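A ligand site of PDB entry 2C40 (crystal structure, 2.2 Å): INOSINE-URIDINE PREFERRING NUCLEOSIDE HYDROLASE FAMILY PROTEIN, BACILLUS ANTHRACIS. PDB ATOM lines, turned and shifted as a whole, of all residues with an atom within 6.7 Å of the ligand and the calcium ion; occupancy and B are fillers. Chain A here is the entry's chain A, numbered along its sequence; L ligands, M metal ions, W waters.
ND2 of Asn 160 sits at hydrogen-bond distance from O1 of the ligand (2.9 Å). The side-chain carboxylate (OE1) of Glu 171 lies within hydrogen-bond range of an oxygen (O1) of the ligand, 2.8 Å away. The side-chain carboxylate (OD1) of Asp 38 sits close to an oxygen (O4) of the ligand (3.2 Å). An oxygen (O3) of the ligand sits close to the side-chain amide nitrogen (ND2) of Asn 173.
The side-chain amide nitrogen (ND2) of Asn 173 lies close to the backbone carbonyl oxygen (O) of Thr 125 (3.1 Å). The backbone NH (N) of Gly 11 lies close to the side-chain carboxylate (OD2) of Asp 14 (3.0 Å). The side-chain carboxylate of Asp 9 sits at hydrogen-bond distance from the backbone NH of Asp 38 (3.0 Å). ND2 of Asn 173 is in hydrogen-bond range of O of Met 151, at 2.9 Å. The backbone NH (N) of Asp 247 lies within hydrogen-bond range of the side-chain carboxylate (OD2) of Asp 13, at 3.5 Å. N of Trp 172 is in hydrogen-bond range of OD1 of Asn 160 (3.0 Å). The side-chain carboxylate (OE1) of Glu 171 lies within hydrogen-bond range of the backbone NH (N) of Asn 173, at 2.7 Å. The side-chain carboxylate (OE2) of Glu 171 sits at hydrogen-bond distance from the side-chain hydroxyl (OG) of Ser 174, 2.9 Å away.
Asp 13 touches the ligand. CE2 of Phe 73 touches O2 of the ligand, 3.7 Å away. Met 151 touches the ligand (SD to C1, 3.8 Å). CB of Trp 172 touches O1 of the ligand (3.4 Å). Hydrophobic or aromatic side chains that line the ligand: Phe 73, Met 151 and Trp 172. 12 residues have an atom within 4 Å of the ligand: Asp 9, Asp 13, Asp 14, Asp 38, Phe 73, Thr 125, Met 151, Asn 160, Glu 171, Trp 172, Asn 173 and Asp 247.
Within 4 Å of the calcium ion: Asp 9, Asp 14, Thr 125 and Asp 247. The nearest printed residue that does not touch the calcium ion is Gly 126 (4.2 Å).
The calcium ion is bound by the side-chain carboxylate (OD2) of Asp 9 (2.3 Å), an oxygen (O4) of the ligand (2.4 Å), the side-chain carboxylate (OD2) of Asp 14 (2.4 Å), the side-chain carboxylate (OD2) of Asp 247 (2.5 Å), water W1 (2.5 Å), the backbone carbonyl oxygen (O) of Thr 125 (2.5 Å), an oxygen (O3) of the ligand (2.7 Å) and the side-chain carboxylate (OD1) of Asp 14 (2.8 Å). The calcium ion has eight donor atoms within binding distance.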
ATOM      1  N   HIS A   8      -7.126  19.311  14.516  1.00  0.00           N
ATOM      2  CA  HIS A   8      -6.297  20.402  15.068  1.00  0.00           C
ATOM      3  C   HIS A   8      -6.505  21.680  14.311  1.00  0.00           C
ATOM      4  O   HIS A   8      -6.995  21.644  13.196  1.00  0.00           O
ATOM      5  CB  HIS A   8      -4.802  20.024  15.119  1.00  0.00           C
ATOM      6  CG  HIS A   8      -4.085  19.982  13.781  1.00  0.00           C
ATOM      7  ND1 HIS A   8      -3.535  21.089  13.180  1.00  0.00           N
ATOM      8  CD2 HIS A   8      -3.743  18.920  12.999  1.00  0.00           C
ATOM      9  CE1 HIS A   8      -2.943  20.727  12.060  1.00  0.00           C
ATOM     10  NE2 HIS A   8      -3.046  19.405  11.925  1.00  0.00           N
ATOM     11  N   ASP A   9      -6.113  22.813  14.896  1.00  0.00           N
ATOM     12  CA  ASP A   9      -6.232  24.077  14.162  1.00  0.00           C
ATOM     13  C   ASP A   9      -4.913  24.784  13.852  1.00  0.00           C
ATOM     14  O   ASP A   9      -4.864  25.976  13.816  1.00  0.00           O
ATOM     15  CB  ASP A   9      -7.226  25.033  14.818  1.00  0.00           C
ATOM     16  CG  ASP A   9      -6.787  25.538  16.148  1.00  0.00           C
ATOM     17  OD1 ASP A   9      -7.386  26.541  16.588  1.00  0.00           O
ATOM     18  OD2 ASP A   9      -5.877  24.943  16.762  1.00  0.00           O
ATOM     19  N   GLY A  10      -3.858  24.006  13.673  1.00  0.00           N
ATOM     20  CA  GLY A  10      -2.643  24.443  12.982  1.00  0.00           C
ATOM     21  C   GLY A  10      -1.827  25.549  13.602  1.00  0.00           C
ATOM     22  O   GLY A  10      -1.038  26.142  12.902  1.00  0.00           O
ATOM     23  N   GLY A  11      -2.023  25.856  14.886  1.00  0.00           N
ATOM     24  CA  GLY A  11      -1.026  26.642  15.649  1.00  0.00           C
ATOM     25  C   GLY A  11       0.269  25.836  15.750  1.00  0.00           C
ATOM     26  O   GLY A  11       0.343  24.679  15.339  1.00  0.00           O
ATOM     27  N   VAL A  12       1.314  26.465  16.252  1.00  0.00           N
ATOM     28  CA  VAL A  12       2.610  25.788  16.457  1.00  0.00           C
ATOM     29  C   VAL A  12       2.459  24.534  17.298  1.00  0.00           C
ATOM     30  O   VAL A  12       3.061  23.501  16.984  1.00  0.00           O
ATOM     31  CB  VAL A  12       3.641  26.754  17.062  1.00  0.00           C
ATOM     32  CG1 VAL A  12       4.824  26.002  17.709  1.00  0.00           C
ATOM     33  CG2 VAL A  12       4.140  27.652  15.981  1.00  0.00           C
ATOM     34  N   ASP A  13       1.673  24.597  18.366  1.00  0.00           N
ATOM     35  CA  ASP A  13       1.600  23.425  19.261  1.00  0.00           C
ATOM     36  C   ASP A  13       0.682  22.297  18.728  1.00  0.00           C
ATOM     37  O   ASP A  13       0.855  21.150  19.129  1.00  0.00           O
ATOM     38  CB  ASP A  13       1.331  23.803  20.748  1.00  0.00           C
ATOM     39  CG  ASP A  13       0.001  24.451  20.971  1.00  0.00           C
ATOM     40  OD1 ASP A  13      -0.773  24.524  19.986  1.00  0.00           O
ATOM     41  OD2 ASP A  13      -0.275  24.877  22.133  1.00  0.00           O
ATOM     42  N   ASP A  14      -0.239  22.634  17.818  1.00  0.00           N
ATOM     43  CA  ASP A  14      -1.009  21.639  17.061  1.00  0.00           C
ATOM     44  C   ASP A  14      -0.087  20.831  16.161  1.00  0.00           C
ATOM     45  O   ASP A  14      -0.197  19.631  16.041  1.00  0.00           O
ATOM     46  CB  ASP A  14      -2.060  22.314  16.170  1.00  0.00           C
ATOM     47  CG  ASP A  14      -3.152  23.010  16.958  1.00  0.00           C
ATOM     48  OD1 ASP A  14      -4.138  22.339  17.373  1.00  0.00           O
ATOM     49  OD2 ASP A  14      -3.042  24.233  17.199  1.00  0.00           O
ATOM     50  N   ASP A  38      -7.214  28.746  14.540  1.00  0.00           N
ATOM     51  CA  ASP A  38      -5.971  29.470  14.829  1.00  0.00           C
ATOM     52  C   ASP A  38      -4.925  29.300  13.723  1.00  0.00           C
ATOM     53  O   ASP A  38      -3.734  29.167  13.985  1.00  0.00           O
ATOM     54  CB  ASP A  38      -5.429  29.015  16.155  1.00  0.00           C
ATOM     55  CG  ASP A  38      -4.422  29.950  16.729  1.00  0.00           C
ATOM     56  OD1 ASP A  38      -3.709  29.463  17.613  1.00  0.00           O
ATOM     57  OD2 ASP A  38      -4.324  31.110  16.296  1.00  0.00           O
ATOM     58  N   PHE A  73     -10.121  33.764  15.413  1.00  0.00           N
ATOM     59  CA  PHE A  73      -8.880  34.047  16.158  1.00  0.00           C
ATOM     60  C   PHE A  73      -8.187  35.297  15.634  1.00  0.00           C
ATOM     61  O   PHE A  73      -8.478  35.740  14.517  1.00  0.00           O
ATOM     62  CB  PHE A  73      -7.910  32.869  16.041  1.00  0.00           C
ATOM     63  CG  PHE A  73      -8.161  31.719  17.004  1.00  0.00           C
ATOM     64  CD1 PHE A  73      -9.111  30.720  16.717  1.00  0.00           C
ATOM     65  CD2 PHE A  73      -7.392  31.564  18.117  1.00  0.00           C
ATOM     66  CE1 PHE A  73      -9.339  29.693  17.544  1.00  0.00           C
ATOM     67  CE2 PHE A  73      -7.581  30.474  18.976  1.00  0.00           C
ATOM     68  CZ  PHE A  73      -8.578  29.556  18.712  1.00  0.00           C
ATOM     69  N   TRP A  77      -1.826  35.448  15.346  1.00  0.00           N
ATOM     70  CA  TRP A  77      -1.692  34.045  15.794  1.00  0.00           C
ATOM     71  C   TRP A  77      -1.873  33.076  14.622  1.00  0.00           C
ATOM     72  O   TRP A  77      -1.143  32.094  14.469  1.00  0.00           O
ATOM     73  CB  TRP A  77      -2.787  33.753  16.825  1.00  0.00           C
ATOM     74  CG  TRP A  77      -2.686  34.519  18.102  1.00  0.00           C
ATOM     75  CD1 TRP A  77      -1.895  35.633  18.359  1.00  0.00           C
ATOM     76  CD2 TRP A  77      -3.443  34.269  19.295  1.00  0.00           C
ATOM     77  NE1 TRP A  77      -2.121  36.053  19.656  1.00  0.00           N
ATOM     78  CE2 TRP A  77      -3.052  35.230  20.253  1.00  0.00           C
ATOM     79  CE3 TRP A  77      -4.405  33.311  19.652  1.00  0.00           C
ATOM     80  CZ2 TRP A  77      -3.598  35.270  21.533  1.00  0.00           C
ATOM     81  CZ3 TRP A  77      -4.934  33.342  20.921  1.00  0.00           C
ATOM     82  CH2 TRP A  77      -4.546  34.310  21.849  1.00  0.00           C
ATOM     83  N   THR A 125      -7.550  19.611  19.369  1.00  0.00           N
ATOM     84  CA  THR A 125      -6.726  20.649  19.885  1.00  0.00           C
ATOM     85  C   THR A 125      -7.042  22.053  19.328  1.00  0.00           C
ATOM     86  O   THR A 125      -6.404  23.008  19.748  1.00  0.00           O
ATOM     87  CB  THR A 125      -5.219  20.319  19.773  1.00  0.00           C
ATOM     88  OG1 THR A 125      -4.791  20.167  18.402  1.00  0.00           O
ATOM     89  CG2 THR A 125      -4.910  19.076  20.562  1.00  0.00           C
ATOM     90  N   GLY A 126      -8.067  22.165  18.493  1.00  0.00           N
ATOM     91  CA  GLY A 126      -8.722  23.404  18.149  1.00  0.00           C
ATOM     92  C   GLY A 126     -10.176  23.377  18.648  1.00  0.00           C
ATOM     93  O   GLY A 126     -10.546  22.557  19.486  1.00  0.00           O
ATOM     94  N   PRO A 127     -11.035  24.294  18.136  1.00  0.00           N
ATOM     95  CA  PRO A 127     -12.475  24.317  18.381  1.00  0.00           C
ATOM     96  C   PRO A 127     -13.192  22.993  18.063  1.00  0.00           C
ATOM     97  O   PRO A 127     -12.620  22.171  17.357  1.00  0.00           O
ATOM     98  CB  PRO A 127     -12.928  25.383  17.392  1.00  0.00           C
ATOM     99  CG  PRO A 127     -11.785  26.306  17.283  1.00  0.00           C
ATOM    100  CD  PRO A 127     -10.629  25.381  17.244  1.00  0.00           C
ATOM    101  N   MET A 151      -8.563  20.067  24.313  1.00  0.00           N
ATOM    102  CA  MET A 151      -8.025  21.301  24.813  1.00  0.00           C
ATOM    103  C   MET A 151      -9.096  22.376  24.708  1.00  0.00           C
ATOM    104  O   MET A 151      -9.417  22.886  23.624  1.00  0.00           O
ATOM    105  CB  MET A 151      -6.767  21.710  24.048  1.00  0.00           C
ATOM    106  CG  MET A 151      -5.894  22.786  24.815  1.00  0.00           C
ATOM    107  SD  MET A 151      -6.557  24.485  24.880  1.00  0.00           S
ATOM    108  CE  MET A 151      -6.495  24.805  26.606  1.00  0.00           C
ATOM    109  N   GLY A 152      -9.643  22.744  25.831  1.00  0.00           N
ATOM    110  CA  GLY A 152     -10.649  23.811  25.864  1.00  0.00           C
ATOM    111  C   GLY A 152     -11.049  24.134  27.282  1.00  0.00           C
ATOM    112  O   GLY A 152     -10.804  23.364  28.236  1.00  0.00           O
ATOM    113  N   ASN A 160      -8.405  33.475  28.308  1.00  0.00           N
ATOM    114  CA  ASN A 160      -7.339  34.061  27.443  1.00  0.00           C
ATOM    115  C   ASN A 160      -7.940  34.761  26.237  1.00  0.00           C
ATOM    116  O   ASN A 160      -7.209  35.217  25.309  1.00  0.00           O
ATOM    117  CB  ASN A 160      -6.392  32.983  26.968  1.00  0.00           C
ATOM    118  CG  ASN A 160      -7.097  31.907  26.135  1.00  0.00           C
ATOM    119  OD1 ASN A 160      -8.325  31.813  26.144  1.00  0.00           O
ATOM    120  ND2 ASN A 160      -6.334  31.122  25.418  1.00  0.00           N
ATOM    121  N   VAL A 161      -9.266  34.914  26.283  1.00  0.00           N
ATOM    122  CA  VAL A 161     -10.001  35.708  25.291  1.00  0.00           C
ATOM    123  C   VAL A 161     -10.161  37.162  25.792  1.00  0.00           C
ATOM    124  O   VAL A 161     -10.825  37.413  26.800  1.00  0.00           O
ATOM    125  CB  VAL A 161     -11.415  35.075  24.994  1.00  0.00           C
ATOM    126  CG1 VAL A 161     -12.181  35.881  24.008  1.00  0.00           C
ATOM    127  CG2 VAL A 161     -11.267  33.708  24.398  1.00  0.00           C
ATOM    128  N   GLU A 171     -12.219  30.624  27.299  1.00  0.00           N
ATOM    129  CA  GLU A 171     -10.998  30.165  26.679  1.00  0.00           C
ATOM    130  C   GLU A 171     -11.271  30.126  25.154  1.00  0.00           C
ATOM    131  O   GLU A 171     -12.419  29.973  24.734  1.00  0.00           O
ATOM    132  CB  GLU A 171     -10.656  28.811  27.273  1.00  0.00           C
ATOM    133  CG  GLU A 171      -9.594  28.048  26.606  1.00  0.00           C
ATOM    134  CD  GLU A 171     -10.060  27.362  25.350  1.00  0.00           C
ATOM    135  OE1 GLU A 171      -9.174  27.259  24.498  1.00  0.00           O
ATOM    136  OE2 GLU A 171     -11.275  26.952  25.207  1.00  0.00           O
ATOM    137  N   TRP A 172     -10.214  30.305  24.348  1.00  0.00           N
ATOM    138  CA  TRP A 172     -10.335  30.493  22.897  1.00  0.00           C
ATOM    139  C   TRP A 172     -10.977  29.376  22.079  1.00  0.00           C
ATOM    140  O   TRP A 172     -11.751  29.643  21.149  1.00  0.00           O
ATOM    141  CB  TRP A 172      -8.959  30.890  22.267  1.00  0.00           C
ATOM    142  CG  TRP A 172      -8.856  32.360  22.000  1.00  0.00           C
ATOM    143  CD1 TRP A 172      -8.109  33.283  22.680  1.00  0.00           C
ATOM    144  CD2 TRP A 172      -9.611  33.098  21.036  1.00  0.00           C
ATOM    145  NE1 TRP A 172      -8.314  34.533  22.164  1.00  0.00           N
ATOM    146  CE2 TRP A 172      -9.240  34.439  21.155  1.00  0.00           C
ATOM    147  CE3 TRP A 172     -10.533  32.720  20.047  1.00  0.00           C
ATOM    148  CZ2 TRP A 172      -9.802  35.439  20.358  1.00  0.00           C
ATOM    149  CZ3 TRP A 172     -11.066  33.689  19.239  1.00  0.00           C
ATOM    150  CH2 TRP A 172     -10.699  35.042  19.398  1.00  0.00           C
ATOM    151  N   ASN A 173     -10.577  28.119  22.298  1.00  0.00           N
ATOM    152  CA  ASN A 173     -11.196  27.019  21.531  1.00  0.00           C
ATOM    153  C   ASN A 173     -12.714  26.932  21.746  1.00  0.00           C
ATOM    154  O   ASN A 173     -13.450  26.629  20.806  1.00  0.00           O
ATOM    155  CB  ASN A 173     -10.506  25.670  21.804  1.00  0.00           C
ATOM    156  CG  ASN A 173      -9.087  25.587  21.176  1.00  0.00           C
ATOM    157  OD1 ASN A 173      -8.757  26.354  20.273  1.00  0.00           O
ATOM    158  ND2 ASN A 173      -8.285  24.626  21.634  1.00  0.00           N
ATOM    159  N   SER A 174     -13.181  27.217  22.968  1.00  0.00           N
ATOM    160  CA  SER A 174     -14.602  27.310  23.258  1.00  0.00           C
ATOM    161  C   SER A 174     -15.219  28.561  22.638  1.00  0.00           C
ATOM    162  O   SER A 174     -16.243  28.488  21.966  1.00  0.00           O
ATOM    163  CB  SER A 174     -14.891  27.345  24.759  1.00  0.00           C
ATOM    164  OG  SER A 174     -14.126  26.383  25.449  1.00  0.00           O
ATOM    165  N   LEU A 196      -7.142  25.693  30.352  1.00  0.00           N
ATOM    166  CA  LEU A 196      -6.033  26.600  30.573  1.00  0.00           C
ATOM    167  C   LEU A 196      -5.214  26.300  31.838  1.00  0.00           C
ATOM    168  O   LEU A 196      -3.967  26.355  31.774  1.00  0.00           O
ATOM    169  CB  LEU A 196      -6.503  28.050  30.568  1.00  0.00           C
ATOM    170  CG  LEU A 196      -7.104  28.553  29.236  1.00  0.00           C
ATOM    171  CD1 LEU A 196      -7.707  29.960  29.418  1.00  0.00           C
ATOM    172  CD2 LEU A 196      -6.084  28.563  28.080  1.00  0.00           C
ATOM    173  N   TYR A 243       5.243  30.473  28.557  1.00  0.00           N
ATOM    174  CA  TYR A 243       4.323  29.927  27.542  1.00  0.00           C
ATOM    175  C   TYR A 243       3.950  28.471  27.892  1.00  0.00           C
ATOM    176  O   TYR A 243       4.770  27.691  28.325  1.00  0.00           O
ATOM    177  CB  TYR A 243       5.016  30.047  26.182  1.00  0.00           C
ATOM    178  CG  TYR A 243       4.399  29.393  24.983  1.00  0.00           C
ATOM    179  CD1 TYR A 243       4.410  27.993  24.830  1.00  0.00           C
ATOM    180  CD2 TYR A 243       3.896  30.166  23.946  1.00  0.00           C
ATOM    181  CE1 TYR A 243       3.868  27.387  23.701  1.00  0.00           C
ATOM    182  CE2 TYR A 243       3.338  29.575  22.806  1.00  0.00           C
ATOM    183  CZ  TYR A 243       3.337  28.201  22.676  1.00  0.00           C
ATOM    184  OH  TYR A 243       2.815  27.652  21.521  1.00  0.00           O
ATOM    185  N   TRP A 246      -0.380  23.829  25.689  1.00  0.00           N
ATOM    186  CA  TRP A 246      -1.697  23.275  25.962  1.00  0.00           C
ATOM    187  C   TRP A 246      -2.074  22.105  25.097  1.00  0.00           C
ATOM    188  O   TRP A 246      -2.527  21.104  25.603  1.00  0.00           O
ATOM    189  CB  TRP A 246      -2.746  24.326  25.737  1.00  0.00           C
ATOM    190  CG  TRP A 246      -2.750  25.306  26.771  1.00  0.00           C
ATOM    191  CD1 TRP A 246      -3.206  25.158  28.023  1.00  0.00           C
ATOM    192  CD2 TRP A 246      -2.281  26.645  26.649  1.00  0.00           C
ATOM    193  NE1 TRP A 246      -3.024  26.324  28.728  1.00  0.00           N
ATOM    194  CE2 TRP A 246      -2.464  27.257  27.901  1.00  0.00           C
ATOM    195  CE3 TRP A 246      -1.667  27.354  25.620  1.00  0.00           C
ATOM    196  CZ2 TRP A 246      -2.106  28.587  28.160  1.00  0.00           C
ATOM    197  CZ3 TRP A 246      -1.295  28.681  25.883  1.00  0.00           C
ATOM    198  CH2 TRP A 246      -1.530  29.276  27.143  1.00  0.00           C
ATOM    199  N   ASP A 247      -1.856  22.252  23.807  1.00  0.00           N
ATOM    200  CA  ASP A 247      -2.188  21.202  22.852  1.00  0.00           C
ATOM    201  C   ASP A 247      -1.259  19.965  22.955  1.00  0.00           C
ATOM    202  O   ASP A 247      -1.709  18.826  22.839  1.00  0.00           O
ATOM    203  CB  ASP A 247      -2.165  21.769  21.442  1.00  0.00           C
ATOM    204  CG  ASP A 247      -3.150  22.932  21.287  1.00  0.00           C
ATOM    205  OD1 ASP A 247      -4.049  23.092  22.163  1.00  0.00           O
ATOM    206  OD2 ASP A 247      -3.076  23.629  20.256  1.00  0.00           O
HETATM  207  O1  LIG L   1      -6.860  28.714  23.915  1.00  0.00           O
HETATM  208  C1  LIG L   1      -5.644  27.956  23.679  1.00  0.00           C
HETATM  209  C2  LIG L   1      -5.634  27.548  22.202  1.00  0.00           C
HETATM  210  O2  LIG L   1      -5.487  28.772  21.446  1.00  0.00           O
HETATM  211  C3  LIG L   1      -4.548  26.562  21.722  1.00  0.00           C
HETATM  212  O3  LIG L   1      -5.205  25.288  21.391  1.00  0.00           O
HETATM  213  C4  LIG L   1      -3.762  27.302  20.542  1.00  0.00           C
HETATM  214  O4  LIG L   1      -3.458  26.665  19.215  1.00  0.00           O
HETATM  215  C5  LIG L   1      -4.566  28.605  20.331  1.00  0.00           C
HETATM  216 CA    CA M   1      -4.772  24.683  18.817  1.00  0.00          CA
HETATM  217  O   HOH W   1      -6.482  26.455  19.026  1.00  0.00           O
